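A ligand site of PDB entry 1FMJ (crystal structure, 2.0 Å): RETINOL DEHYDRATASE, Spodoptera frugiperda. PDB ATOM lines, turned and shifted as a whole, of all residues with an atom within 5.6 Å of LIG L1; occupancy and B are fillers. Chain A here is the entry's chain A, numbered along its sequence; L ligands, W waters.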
ATOM      1  N   SER A  70       1.488  16.642 -19.492  1.00  0.00           N
ATOM      2  CA  SER A  70       2.872  16.304 -19.202  1.00  0.00           C
ATOM      3  C   SER A  70       3.766  17.476 -19.488  1.00  0.00           C
ATOM      4  O   SER A  70       3.347  18.438 -20.134  1.00  0.00           O
ATOM      5  CB  SER A  70       3.336  15.180 -20.115  1.00  0.00           C
ATOM      6  OG  SER A  70       3.330  15.666 -21.449  1.00  0.00           O
ATOM      7  N   TYR A  71       5.010  17.391 -19.026  1.00  0.00           N
ATOM      8  CA  TYR A  71       5.966  18.419 -19.398  1.00  0.00           C
ATOM      9  C   TYR A  71       6.373  17.792 -20.748  1.00  0.00           C
ATOM     10  O   TYR A  71       6.523  16.572 -20.839  1.00  0.00           O
ATOM     11  CB  TYR A  71       7.179  18.471 -18.478  1.00  0.00           C
ATOM     12  CG  TYR A  71       8.150  19.485 -19.017  1.00  0.00           C
ATOM     13  CD1 TYR A  71       7.960  20.843 -18.786  1.00  0.00           C
ATOM     14  CD2 TYR A  71       9.151  19.106 -19.916  1.00  0.00           C
ATOM     15  CE1 TYR A  71       8.735  21.812 -19.447  1.00  0.00           C
ATOM     16  CE2 TYR A  71       9.919  20.052 -20.574  1.00  0.00           C
ATOM     17  CZ  TYR A  71       9.695  21.402 -20.349  1.00  0.00           C
ATOM     18  OH  TYR A  71      10.396  22.331 -21.078  1.00  0.00           O
ATOM     19  N   GLN A  72       6.543  18.593 -21.775  1.00  0.00           N
ATOM     20  CA  GLN A  72       6.861  18.045 -23.103  1.00  0.00           C
ATOM     21  C   GLN A  72       8.018  17.060 -23.208  1.00  0.00           C
ATOM     22  O   GLN A  72       8.999  17.146 -22.482  1.00  0.00           O
ATOM     23  CB  GLN A  72       7.098  19.184 -24.111  1.00  0.00           C
ATOM     24  CG  GLN A  72       8.276  20.093 -23.791  1.00  0.00           C
ATOM     25  CD  GLN A  72       8.769  20.854 -25.016  1.00  0.00           C
ATOM     26  OE1 GLN A  72       9.849  20.569 -25.542  1.00  0.00           O
ATOM     27  NE2 GLN A  72       7.974  21.811 -25.479  1.00  0.00           N
ATOM     28  N   ARG A  73       7.858  16.115 -24.140  1.00  0.00           N
ATOM     29  CA  ARG A  73       8.845  15.083 -24.436  1.00  0.00           C
ATOM     30  C   ARG A  73       8.962  14.050 -23.331  1.00  0.00           C
ATOM     31  O   ARG A  73      10.012  13.431 -23.155  1.00  0.00           O
ATOM     32  CB  ARG A  73      10.216  15.736 -24.713  1.00  0.00           C
ATOM     33  CG  ARG A  73      10.162  16.812 -25.795  1.00  0.00           C
ATOM     34  CD  ARG A  73       9.473  16.323 -27.063  1.00  0.00           C
ATOM     35  NE  ARG A  73      10.318  15.458 -27.895  1.00  0.00           N
ATOM     36  CZ  ARG A  73       9.864  14.754 -28.918  1.00  0.00           C
ATOM     37  NH1 ARG A  73       8.581  14.811 -29.231  1.00  0.00           N
ATOM     38  NH2 ARG A  73      10.686  14.017 -29.661  1.00  0.00           N
ATOM     39  N   SER A  74       7.880  13.857 -22.592  1.00  0.00           N
ATOM     40  CA  SER A  74       7.858  12.908 -21.494  1.00  0.00           C
ATOM     41  C   SER A  74       7.044  11.656 -21.773  1.00  0.00           C
ATOM     42  O   SER A  74       6.840  10.845 -20.882  1.00  0.00           O
ATOM     43  CB  SER A  74       7.299  13.588 -20.238  1.00  0.00           C
ATOM     44  OG  SER A  74       8.116  14.661 -19.835  1.00  0.00           O
ATOM     45  N   GLY A  75       6.565  11.519 -23.006  1.00  0.00           N
ATOM     46  CA  GLY A  75       5.771  10.334 -23.351  1.00  0.00           C
ATOM     47  C   GLY A  75       4.298  10.599 -23.651  1.00  0.00           C
ATOM     48  O   GLY A  75       3.471   9.703 -23.565  1.00  0.00           O
ATOM     49  N   THR A  76       3.980  11.835 -24.022  1.00  0.00           N
ATOM     50  CA  THR A  76       2.596  12.203 -24.315  1.00  0.00           C
ATOM     51  C   THR A  76       1.983  11.467 -25.518  1.00  0.00           C
ATOM     52  O   THR A  76       0.852  10.998 -25.444  1.00  0.00           O
ATOM     53  CB  THR A  76       2.484  13.725 -24.568  1.00  0.00           C
ATOM     54  OG1 THR A  76       3.313  14.418 -23.638  1.00  0.00           O
ATOM     55  CG2 THR A  76       1.040  14.195 -24.398  1.00  0.00           C
ATOM     56  N   THR A  77       2.726  11.384 -26.610  1.00  0.00           N
ATOM     57  CA  THR A  77       2.208  10.742 -27.827  1.00  0.00           C
ATOM     58  C   THR A  77       1.781   9.300 -27.603  1.00  0.00           C
ATOM     59  O   THR A  77       0.695   8.910 -28.016  1.00  0.00           O
ATOM     60  CB  THR A  77       3.236  10.791 -28.973  1.00  0.00           C
ATOM     61  OG1 THR A  77       3.799  12.101 -29.046  1.00  0.00           O
ATOM     62  CG2 THR A  77       2.556  10.481 -30.298  1.00  0.00           C
ATOM     63  N   MET A  78       2.640   8.511 -26.953  1.00  0.00           N
ATOM     64  CA  MET A  78       2.349   7.119 -26.644  1.00  0.00           C
ATOM     65  C   MET A  78       1.056   7.035 -25.882  1.00  0.00           C
ATOM     66  O   MET A  78       0.133   6.299 -26.240  1.00  0.00           O
ATOM     67  CB  MET A  78       3.428   6.510 -25.746  1.00  0.00           C
ATOM     68  CG  MET A  78       4.815   6.551 -26.299  1.00  0.00           C
ATOM     69  SD  MET A  78       5.948   6.039 -25.031  1.00  0.00           S
ATOM     70  CE  MET A  78       5.573   4.273 -24.967  1.00  0.00           C
ATOM     71  N   HIS A 164       0.402  20.670 -22.208  1.00  0.00           N
ATOM     72  CA  HIS A 164       1.658  20.725 -21.498  1.00  0.00           C
ATOM     73  C   HIS A 164       1.505  21.812 -20.423  1.00  0.00           C
ATOM     74  O   HIS A 164       2.472  22.280 -19.855  1.00  0.00           O
ATOM     75  CB  HIS A 164       2.828  21.032 -22.438  1.00  0.00           C
ATOM     76  CG  HIS A 164       3.021  20.005 -23.512  1.00  0.00           C
ATOM     77  ND1 HIS A 164       3.123  18.656 -23.234  1.00  0.00           N
ATOM     78  CD2 HIS A 164       3.118  20.121 -24.861  1.00  0.00           C
ATOM     79  CE1 HIS A 164       3.265  17.985 -24.368  1.00  0.00           C
ATOM     80  NE2 HIS A 164       3.282  18.853 -25.364  1.00  0.00           N
ATOM     81  N   ARG A 185       9.059  12.138 -16.779  1.00  0.00           N
ATOM     82  CA  ARG A 185      10.209  11.415 -17.284  1.00  0.00           C
ATOM     83  C   ARG A 185      11.464  12.063 -16.712  1.00  0.00           C
ATOM     84  O   ARG A 185      11.466  13.247 -16.416  1.00  0.00           O
ATOM     85  CB  ARG A 185      10.222  11.523 -18.820  1.00  0.00           C
ATOM     86  CG  ARG A 185      11.314  10.732 -19.518  1.00  0.00           C
ATOM     87  CD  ARG A 185      11.316  11.027 -21.011  1.00  0.00           C
ATOM     88  NE  ARG A 185      12.302  10.219 -21.728  1.00  0.00           N
ATOM     89  CZ  ARG A 185      12.584  10.320 -23.016  1.00  0.00           C
ATOM     90  NH1 ARG A 185      11.945  11.211 -23.784  1.00  0.00           N
ATOM     91  NH2 ARG A 185      13.498   9.523 -23.553  1.00  0.00           N
ATOM     92  N   ASP A 189      16.788  13.310 -19.689  1.00  0.00           N
ATOM     93  CA  ASP A 189      16.410  12.783 -20.998  1.00  0.00           C
ATOM     94  C   ASP A 189      15.375  13.706 -21.652  1.00  0.00           C
ATOM     95  O   ASP A 189      15.287  13.792 -22.873  1.00  0.00           O
ATOM     96  CB  ASP A 189      15.813  11.373 -20.873  1.00  0.00           C
ATOM     97  CG  ASP A 189      16.853  10.331 -20.519  1.00  0.00           C
ATOM     98  OD1 ASP A 189      17.993  10.470 -21.006  1.00  0.00           O
ATOM     99  OD2 ASP A 189      16.517   9.381 -19.778  1.00  0.00           O
ATOM    100  N   VAL A 192      17.343  16.417 -23.269  1.00  0.00           N
ATOM    101  CA  VAL A 192      17.909  15.944 -24.535  1.00  0.00           C
ATOM    102  C   VAL A 192      16.803  15.862 -25.603  1.00  0.00           C
ATOM    103  O   VAL A 192      16.982  16.320 -26.727  1.00  0.00           O
ATOM    104  CB  VAL A 192      18.574  14.558 -24.390  1.00  0.00           C
ATOM    105  CG1 VAL A 192      18.976  14.001 -25.773  1.00  0.00           C
ATOM    106  CG2 VAL A 192      19.815  14.671 -23.536  1.00  0.00           C
ATOM    107  N   SER A 193      15.660  15.291 -25.236  1.00  0.00           N
ATOM    108  CA  SER A 193      14.582  15.180 -26.219  1.00  0.00           C
ATOM    109  C   SER A 193      14.022  16.549 -26.589  1.00  0.00           C
ATOM    110  O   SER A 193      13.616  16.772 -27.733  1.00  0.00           O
ATOM    111  CB  SER A 193      13.460  14.282 -25.698  1.00  0.00           C
ATOM    112  OG  SER A 193      12.472  14.093 -26.716  1.00  0.00           O
ATOM    113  N   TYR A 248       7.516   7.692 -17.783  1.00  0.00           N
ATOM    114  CA  TYR A 248       7.895   7.216 -19.113  1.00  0.00           C
ATOM    115  C   TYR A 248       8.765   5.959 -19.034  1.00  0.00           C
ATOM    116  O   TYR A 248       8.647   5.064 -19.865  1.00  0.00           O
ATOM    117  CB  TYR A 248       8.641   8.318 -19.851  1.00  0.00           C
ATOM    118  CG  TYR A 248       9.279   7.868 -21.146  1.00  0.00           C
ATOM    119  CD1 TYR A 248       8.517   7.603 -22.281  1.00  0.00           C
ATOM    120  CD2 TYR A 248      10.658   7.705 -21.226  1.00  0.00           C
ATOM    121  CE1 TYR A 248       9.116   7.184 -23.469  1.00  0.00           C
ATOM    122  CE2 TYR A 248      11.263   7.295 -22.397  1.00  0.00           C
ATOM    123  CZ  TYR A 248      10.496   7.038 -23.510  1.00  0.00           C
ATOM    124  OH  TYR A 248      11.127   6.642 -24.675  1.00  0.00           O
ATOM    125  N   LEU A 252       8.746   1.558 -20.759  1.00  0.00           N
ATOM    126  CA  LEU A 252       9.830   0.773 -21.349  1.00  0.00           C
ATOM    127  C   LEU A 252      10.148  -0.489 -20.549  1.00  0.00           C
ATOM    128  O   LEU A 252      10.694  -1.453 -21.100  1.00  0.00           O
ATOM    129  CB  LEU A 252      11.094   1.626 -21.466  1.00  0.00           C
ATOM    130  CG  LEU A 252      10.967   3.003 -22.106  1.00  0.00           C
ATOM    131  CD1 LEU A 252      12.337   3.673 -22.164  1.00  0.00           C
ATOM    132  CD2 LEU A 252      10.386   2.869 -23.512  1.00  0.00           C
ATOM    133  N   LEU A 282       2.510  -0.272 -30.016  1.00  0.00           N
ATOM    134  CA  LEU A 282       3.359   0.824 -29.591  1.00  0.00           C
ATOM    135  C   LEU A 282       4.833   0.511 -29.732  1.00  0.00           C
ATOM    136  O   LEU A 282       5.673   1.213 -29.167  1.00  0.00           O
ATOM    137  CB  LEU A 282       3.077   1.199 -28.133  1.00  0.00           C
ATOM    138  CG  LEU A 282       1.717   1.753 -27.706  1.00  0.00           C
ATOM    139  CD1 LEU A 282       1.952   2.665 -26.516  1.00  0.00           C
ATOM    140  CD2 LEU A 282       1.053   2.536 -28.828  1.00  0.00           C
ATOM    141  N   ASN A 283       5.165  -0.565 -30.447  1.00  0.00           N
ATOM    142  CA  ASN A 283       6.569  -0.915 -30.647  1.00  0.00           C
ATOM    143  C   ASN A 283       7.224   0.314 -31.255  1.00  0.00           C
ATOM    144  O   ASN A 283       6.687   0.907 -32.193  1.00  0.00           O
ATOM    145  CB  ASN A 283       6.687  -2.103 -31.599  1.00  0.00           C
ATOM    146  CG  ASN A 283       8.120  -2.436 -31.951  1.00  0.00           C
ATOM    147  OD1 ASN A 283       8.736  -1.759 -32.782  1.00  0.00           O
ATOM    148  ND2 ASN A 283       8.654  -3.464 -31.321  1.00  0.00           N
ATOM    149  N   PHE A 284       8.394   0.710 -30.749  1.00  0.00           N
ATOM    150  CA  PHE A 284       9.041   1.915 -31.247  1.00  0.00           C
ATOM    151  C   PHE A 284       9.192   2.046 -32.744  1.00  0.00           C
ATOM    152  O   PHE A 284       8.857   3.091 -33.300  1.00  0.00           O
ATOM    153  CB  PHE A 284      10.412   2.132 -30.617  1.00  0.00           C
ATOM    154  CG  PHE A 284      11.000   3.484 -30.948  1.00  0.00           C
ATOM    155  CD1 PHE A 284      10.436   4.642 -30.427  1.00  0.00           C
ATOM    156  CD2 PHE A 284      12.081   3.581 -31.818  1.00  0.00           C
ATOM    157  CE1 PHE A 284      10.952   5.895 -30.762  1.00  0.00           C
ATOM    158  CE2 PHE A 284      12.604   4.828 -32.153  1.00  0.00           C
ATOM    159  CZ  PHE A 284      12.028   5.986 -31.626  1.00  0.00           C
ATOM    160  N   PHE A 287       5.598   2.275 -34.296  1.00  0.00           N
ATOM    161  CA  PHE A 287       5.068   3.578 -33.920  1.00  0.00           C
ATOM    162  C   PHE A 287       5.790   4.698 -34.681  1.00  0.00           C
ATOM    163  O   PHE A 287       5.171   5.615 -35.232  1.00  0.00           O
ATOM    164  CB  PHE A 287       5.217   3.779 -32.414  1.00  0.00           C
ATOM    165  CG  PHE A 287       4.235   4.744 -31.824  1.00  0.00           C
ATOM    166  CD1 PHE A 287       2.887   4.422 -31.744  1.00  0.00           C
ATOM    167  CD2 PHE A 287       4.653   5.983 -31.337  1.00  0.00           C
ATOM    168  CE1 PHE A 287       1.976   5.315 -31.184  1.00  0.00           C
ATOM    169  CE2 PHE A 287       3.755   6.876 -30.782  1.00  0.00           C
ATOM    170  CZ  PHE A 287       2.411   6.543 -30.710  1.00  0.00           C
ATOM    171  N   PHE A 310       9.966  13.625 -34.968  1.00  0.00           N
ATOM    172  CA  PHE A 310       9.102  13.752 -33.799  1.00  0.00           C
ATOM    173  C   PHE A 310       9.251  12.524 -32.909  1.00  0.00           C
ATOM    174  O   PHE A 310       9.303  12.641 -31.690  1.00  0.00           O
ATOM    175  CB  PHE A 310       7.641  13.907 -34.253  1.00  0.00           C
ATOM    176  CG  PHE A 310       6.720  14.272 -33.142  1.00  0.00           C
ATOM    177  CD1 PHE A 310       6.852  15.487 -32.475  1.00  0.00           C
ATOM    178  CD2 PHE A 310       5.720  13.377 -32.733  1.00  0.00           C
ATOM    179  CE1 PHE A 310       6.010  15.807 -31.411  1.00  0.00           C
ATOM    180  CE2 PHE A 310       4.878  13.696 -31.669  1.00  0.00           C
ATOM    181  CZ  PHE A 310       5.036  14.911 -31.013  1.00  0.00           C
ATOM    182  N   ILE A 311       9.281  11.344 -33.518  1.00  0.00           N
ATOM    183  CA  ILE A 311       9.488  10.090 -32.782  1.00  0.00           C
ATOM    184  C   ILE A 311      10.948   9.789 -33.126  1.00  0.00           C
ATOM    185  O   ILE A 311      11.258   9.358 -34.234  1.00  0.00           O
ATOM    186  CB  ILE A 311       8.533   8.993 -33.281  1.00  0.00           C
ATOM    187  CG1 ILE A 311       7.091   9.422 -32.973  1.00  0.00           C
ATOM    188  CG2 ILE A 311       8.837   7.668 -32.587  1.00  0.00           C
ATOM    189  CD1 ILE A 311       6.048   8.439 -33.445  1.00  0.00           C
ATOM    190  N   ARG A 312      11.826  10.019 -32.153  1.00  0.00           N
ATOM    191  CA  ARG A 312      13.272   9.933 -32.335  1.00  0.00           C
ATOM    192  C   ARG A 312      14.052   8.667 -31.952  1.00  0.00           C
ATOM    193  O   ARG A 312      14.423   7.879 -32.826  1.00  0.00           O
ATOM    194  CB  ARG A 312      13.888  11.144 -31.642  1.00  0.00           C
ATOM    195  CG  ARG A 312      15.332  11.498 -31.993  1.00  0.00           C
ATOM    196  CD  ARG A 312      15.733  12.781 -31.270  1.00  0.00           C
ATOM    197  NE  ARG A 312      15.707  12.595 -29.821  1.00  0.00           N
ATOM    198  CZ  ARG A 312      16.703  12.071 -29.109  1.00  0.00           C
ATOM    199  NH1 ARG A 312      17.812  11.682 -29.727  1.00  0.00           N
ATOM    200  NH2 ARG A 312      16.576  11.905 -27.794  1.00  0.00           N
ATOM    201  N   LYS A 313      14.299   8.490 -30.658  1.00  0.00           N
ATOM    202  CA  LYS A 313      15.077   7.360 -30.139  1.00  0.00           C
ATOM    203  C   LYS A 313      14.273   6.343 -29.323  1.00  0.00           C
ATOM    204  O   LYS A 313      14.336   5.143 -29.591  1.00  0.00           O
ATOM    205  CB  LYS A 313      16.224   7.887 -29.283  1.00  0.00           C
ATOM    206  CG  LYS A 313      17.607   7.785 -29.895  1.00  0.00           C
ATOM    207  CD  LYS A 313      18.214   6.408 -29.671  1.00  0.00           C
ATOM    208  CE  LYS A 313      19.707   6.375 -29.982  1.00  0.00           C
ATOM    209  NZ  LYS A 313      20.026   6.641 -31.427  1.00  0.00           N
ATOM    210  N   GLY A 314      13.557   6.808 -28.312  1.00  0.00           N
ATOM    211  CA  GLY A 314      12.750   5.926 -27.490  1.00  0.00           C
ATOM    212  C   GLY A 314      13.452   5.219 -26.351  1.00  0.00           C
ATOM    213  O   GLY A 314      12.923   4.259 -25.798  1.00  0.00           O
ATOM    214  N   LYS A 315      14.628   5.682 -25.964  1.00  0.00           N
ATOM    215  CA  LYS A 315      15.356   5.035 -24.877  1.00  0.00           C
ATOM    216  C   LYS A 315      15.338   5.868 -23.612  1.00  0.00           C
ATOM    217  O   LYS A 315      14.963   7.041 -23.618  1.00  0.00           O
ATOM    218  CB  LYS A 315      16.826   4.807 -25.272  1.00  0.00           C
ATOM    219  CG  LYS A 315      17.041   4.232 -26.663  1.00  0.00           C
ATOM    220  CD  LYS A 315      16.432   2.852 -26.810  1.00  0.00           C
ATOM    221  CE  LYS A 315      16.767   2.264 -28.185  1.00  0.00           C
ATOM    222  NZ  LYS A 315      16.091   0.957 -28.387  1.00  0.00           N
HETATM  223  P1  LIG L   1      13.197  10.672 -27.319  1.00  0.00           P
HETATM  224  O1  LIG L   1      13.470  12.010 -27.856  1.00  0.00           O
HETATM  225  O2  LIG L   1      13.326   9.634 -28.361  1.00  0.00           O
HETATM  226  O3  LIG L   1      14.103  10.369 -26.202  1.00  0.00           O
HETATM  227  P2  LIG L   1       6.216  13.428 -26.211  1.00  0.00           P
HETATM  228  O4  LIG L   1       5.252  12.610 -26.963  1.00  0.00           O
HETATM  229  O5  LIG L   1       5.663  13.809 -24.892  1.00  0.00           O
HETATM  230  O6  LIG L   1       6.574  14.632 -27.003  1.00  0.00           O
HETATM  231  O7  LIG L   1       7.526  12.576 -25.969  1.00  0.00           O
HETATM  232  C1  LIG L   1       8.309  12.081 -27.041  1.00  0.00           C
HETATM  233  C2  LIG L   1       9.346  11.068 -26.545  1.00  0.00           C
HETATM  234  O8  LIG L   1       8.700   9.767 -26.490  1.00  0.00           O
HETATM  235  C3  LIG L   1      10.516  10.915 -27.508  1.00  0.00           C
HETATM  236  O9  LIG L   1      11.714  10.641 -26.742  1.00  0.00           O
HETATM  237  C4  LIG L   1      10.017   9.793 -28.400  1.00  0.00           C
HETATM  238  O10 LIG L   1      10.941   9.172 -29.291  1.00  0.00           O
HETATM  239  C5  LIG L   1       9.409   8.867 -27.354  1.00  0.00           C
HETATM  240  N1  LIG L   1       8.473   7.900 -27.938  1.00  0.00           N
HETATM  241  C6  LIG L   1       7.433   8.095 -28.838  1.00  0.00           C
HETATM  242  N2  LIG L   1       6.776   7.008 -29.170  1.00  0.00           N
HETATM  243  C7  LIG L   1       7.418   6.013 -28.446  1.00  0.00           C
HETATM  244  C8  LIG L   1       7.206   4.590 -28.333  1.00  0.00           C
HETATM  245  N3  LIG L   1       6.252   3.937 -28.993  1.00  0.00           N
HETATM  246  N4  LIG L   1       8.056   3.868 -27.486  1.00  0.00           N
HETATM  247  C9  LIG L   1       9.049   4.505 -26.787  1.00  0.00           C
HETATM  248  N5  LIG L   1       9.340   5.837 -26.816  1.00  0.00           N
HETATM  249  C10 LIG L   1       8.481   6.548 -27.666  1.00  0.00           C
HETATM  250  C1  LG2 L   2       6.478  26.748 -36.360  1.00  0.00           C
HETATM  251  C2  LG2 L   2       6.754  28.275 -36.527  1.00  0.00           C
HETATM  252  C3  LG2 L   2       5.476  29.105 -36.652  1.00  0.00           C
HETATM  253  C4  LG2 L   2       3.995  28.750 -36.690  1.00  0.00           C
HETATM  254  C5  LG2 L   2       3.923  27.229 -36.529  1.00  0.00           C
HETATM  255  C6  LG2 L   2       4.976  26.308 -36.371  1.00  0.00           C
HETATM  256  C7  LG2 L   2       4.746  24.848 -36.208  1.00  0.00           C
HETATM  257  C8  LG2 L   2       4.428  24.245 -35.026  1.00  0.00           C
HETATM  258  C9  LG2 L   2       4.202  22.806 -34.852  1.00  0.00           C
HETATM  259  C10 LG2 L   2       3.893  22.351 -33.580  1.00  0.00           C
HETATM  260  C11 LG2 L   2       3.619  20.982 -33.099  1.00  0.00           C
HETATM  261  C12 LG2 L   2       4.329  20.698 -31.957  1.00  0.00           C
HETATM  262  C13 LG2 L   2       4.454  19.534 -31.053  1.00  0.00           C
HETATM  263  C14 LG2 L   2       5.178  19.296 -29.916  1.00  0.00           C
HETATM  264  C15 LG2 L   2       4.558  19.538 -28.608  1.00  0.00           C
HETATM  265  O1  LG2 L   2       3.881  18.436 -28.149  1.00  0.00           O
HETATM  266  C16 LG2 L   2       7.196  26.505 -35.015  1.00  0.00           C
HETATM  267  C17 LG2 L   2       7.341  26.130 -37.476  1.00  0.00           C
HETATM  268  C18 LG2 L   2       2.455  26.782 -36.587  1.00  0.00           C
HETATM  269  C19 LG2 L   2       4.322  21.863 -36.069  1.00  0.00           C
HETATM  270  C20 LG2 L   2       3.540  18.438 -31.618  1.00  0.00           C
HETATM  271  O   HOH W   1      15.865   8.170 -26.282  1.00  0.00           O
HETATM  272  O   HOH W   2       5.658  17.129 -26.234  1.00  0.00           O
HETATM  273  O   HOH W   3      16.082  11.758 -24.715  1.00  0.00           O
HETATM  274  O   HOH W   4       8.438   1.038 -27.105  1.00  0.00           O
HETATM  275  O   HOH W   5       6.785  11.574 -29.965  1.00  0.00           O
HETATM  276  O   HOH W   6      13.369  14.724 -29.597  1.00  0.00           O
HETATM  277  O   HOH W   7       5.645   9.701 -26.607  1.00  0.00           O
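An oxygen (O1) of LIG L1 sits at hydrogen-bond distance from the side-chain hydroxyl (OG) of Ser 193. The backbone NH of Thr 77 is in hydrogen-bond range of an oxygen (O4) of LIG L1 (2.8 Å). The side-chain hydroxyl of Thr 77 sits at hydrogen-bond distance from an oxygen (O4) of LIG L1, at 2.6 Å. The backbone NH of Thr 76 is in hydrogen-bond range of an oxygen (O5) of LIG L1 (2.7 Å). An oxygen (O5) of LIG L1 is in hydrogen-bond range of the side-chain hydroxyl (OG1) of Thr 76, 2.7 Å away. N of Lys 313 is in hydrogen-bond range of O2 of LIG L1. A nitrogen (N3) of LIG L1 sits at hydrogen-bond distance from the backbone carbonyl oxygen of Leu 282 (2.8 Å). N of Gly 314 sits at hydrogen-bond distance from O2 of LIG L1 (2.8 Å). An oxygen (O3) of LIG L1 lies within salt-bridge range of the guanidinium group of Arg 185, at 2.8 Å. OH of Tyr 248 lies within hydrogen-bond range of N5 of LIG L1, 2.9 Å away. The backbone NH (N) of Arg 73 lies within hydrogen-bond range of an oxygen (O5) of LIG L1 (3.3 Å). The guanidinium group of Arg 73 lies within salt-bridge range of an oxygen (O6) of LIG L1 (3.0 Å). N of Arg 312 lies within hydrogen-bond range of O10 of LIG L1 (3.1 Å). O1 of LIG L1 lies within salt-bridge range of NE of Arg 312 (3.0 Å). O5 of LIG L1 sits at hydrogen-bond distance from N of Gly 75 (3.1 Å). N of Ser 74 sits at hydrogen-bond distance from O5 of LIG L1, 3.2 Å away. O1 of LG2 L2 lies within hydrogen-bond range of NE2 of His 164 (2.9 Å).
The guanidinium group of Arg 73 is in hydrogen-bond range of the side-chain hydroxyl of Ser 193. The side-chain hydroxyl (OG1) of Thr 76 sits at hydrogen-bond distance from the side-chain hydroxyl (OG) of Ser 70. The backbone carbonyl oxygen (O) of Gly 314 sits at hydrogen-bond distance from the side-chain hydroxyl (OH) of Tyr 248. The guanidinium group (NH1) of Arg 185 is in hydrogen-bond range of the backbone carbonyl oxygen (O) of Arg 73 (3.0 Å). NH2 of Arg 185 lies within hydrogen-bond range of O of Lys 315 (2.9 Å). The guanidinium group (NH2) of Arg 73 lies within hydrogen-bond range of the backbone carbonyl oxygen (O) of Phe 310 (2.8 Å). The side-chain hydroxyl (OG) of Ser 74 is in hydrogen-bond range of the backbone carbonyl oxygen (O) of Tyr 71, 2.7 Å away.
Met 78 touches LIG L1. Leu 252 touches LIG L1. CE1 of Phe 284 touches O10 of LIG L1 (3.6 Å). Phe 287 touches LIG L1. Ile 311 touches LIG L1. Hydrophobic or aromatic side chains that line LIG L1: Met 78, Tyr 248, Leu 252, Phe 284 and Phe 287. 17 residues have an atom within 4 Å of LIG L1: Arg 73, Ser 74, Gly 75, Thr 76, Thr 77, Met 78, Arg 185, Ser 193, Tyr 248, Leu 252, Leu 282, Phe 284, Phe 287, Ile 311, Arg 312, Lys 313 and Gly 314.
Water W1 lies within hydrogen-bond range of the backbone NH (N) of Lys 315 (2.8 Å), an oxygen (O3) of LIG L1 (2.8 Å) and the backbone NH (N) of Gly 314 (3.4 Å). Water W3 lies within hydrogen-bond range of O3 of LIG L1 (2.8 Å), O of Asp 189 (2.9 Å) and NH2 of Arg 312 (3.1 Å). Water W4 bridges a nitrogen (N4) of LIG L1 and the backbone carbonyl oxygen of Leu 282. Water W7 lies within hydrogen-bond range of an oxygen (O4) of LIG L1 (3.0 Å), the backbone NH (N) of Met 78 (3.3 Å) and the backbone NH (N) of Thr 77 (3.4 Å). Water W6 lies within hydrogen-bond range of NH2 of Arg 73 (2.8 Å), O of Ser 193 (2.8 Å), NE of Arg 312 (3.2 Å) and O1 of LIG L1 (3.2 Å). Water W5 bridges OG1 of Thr 77 (3.2 Å) and O of Phe 310 (3.2 Å).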
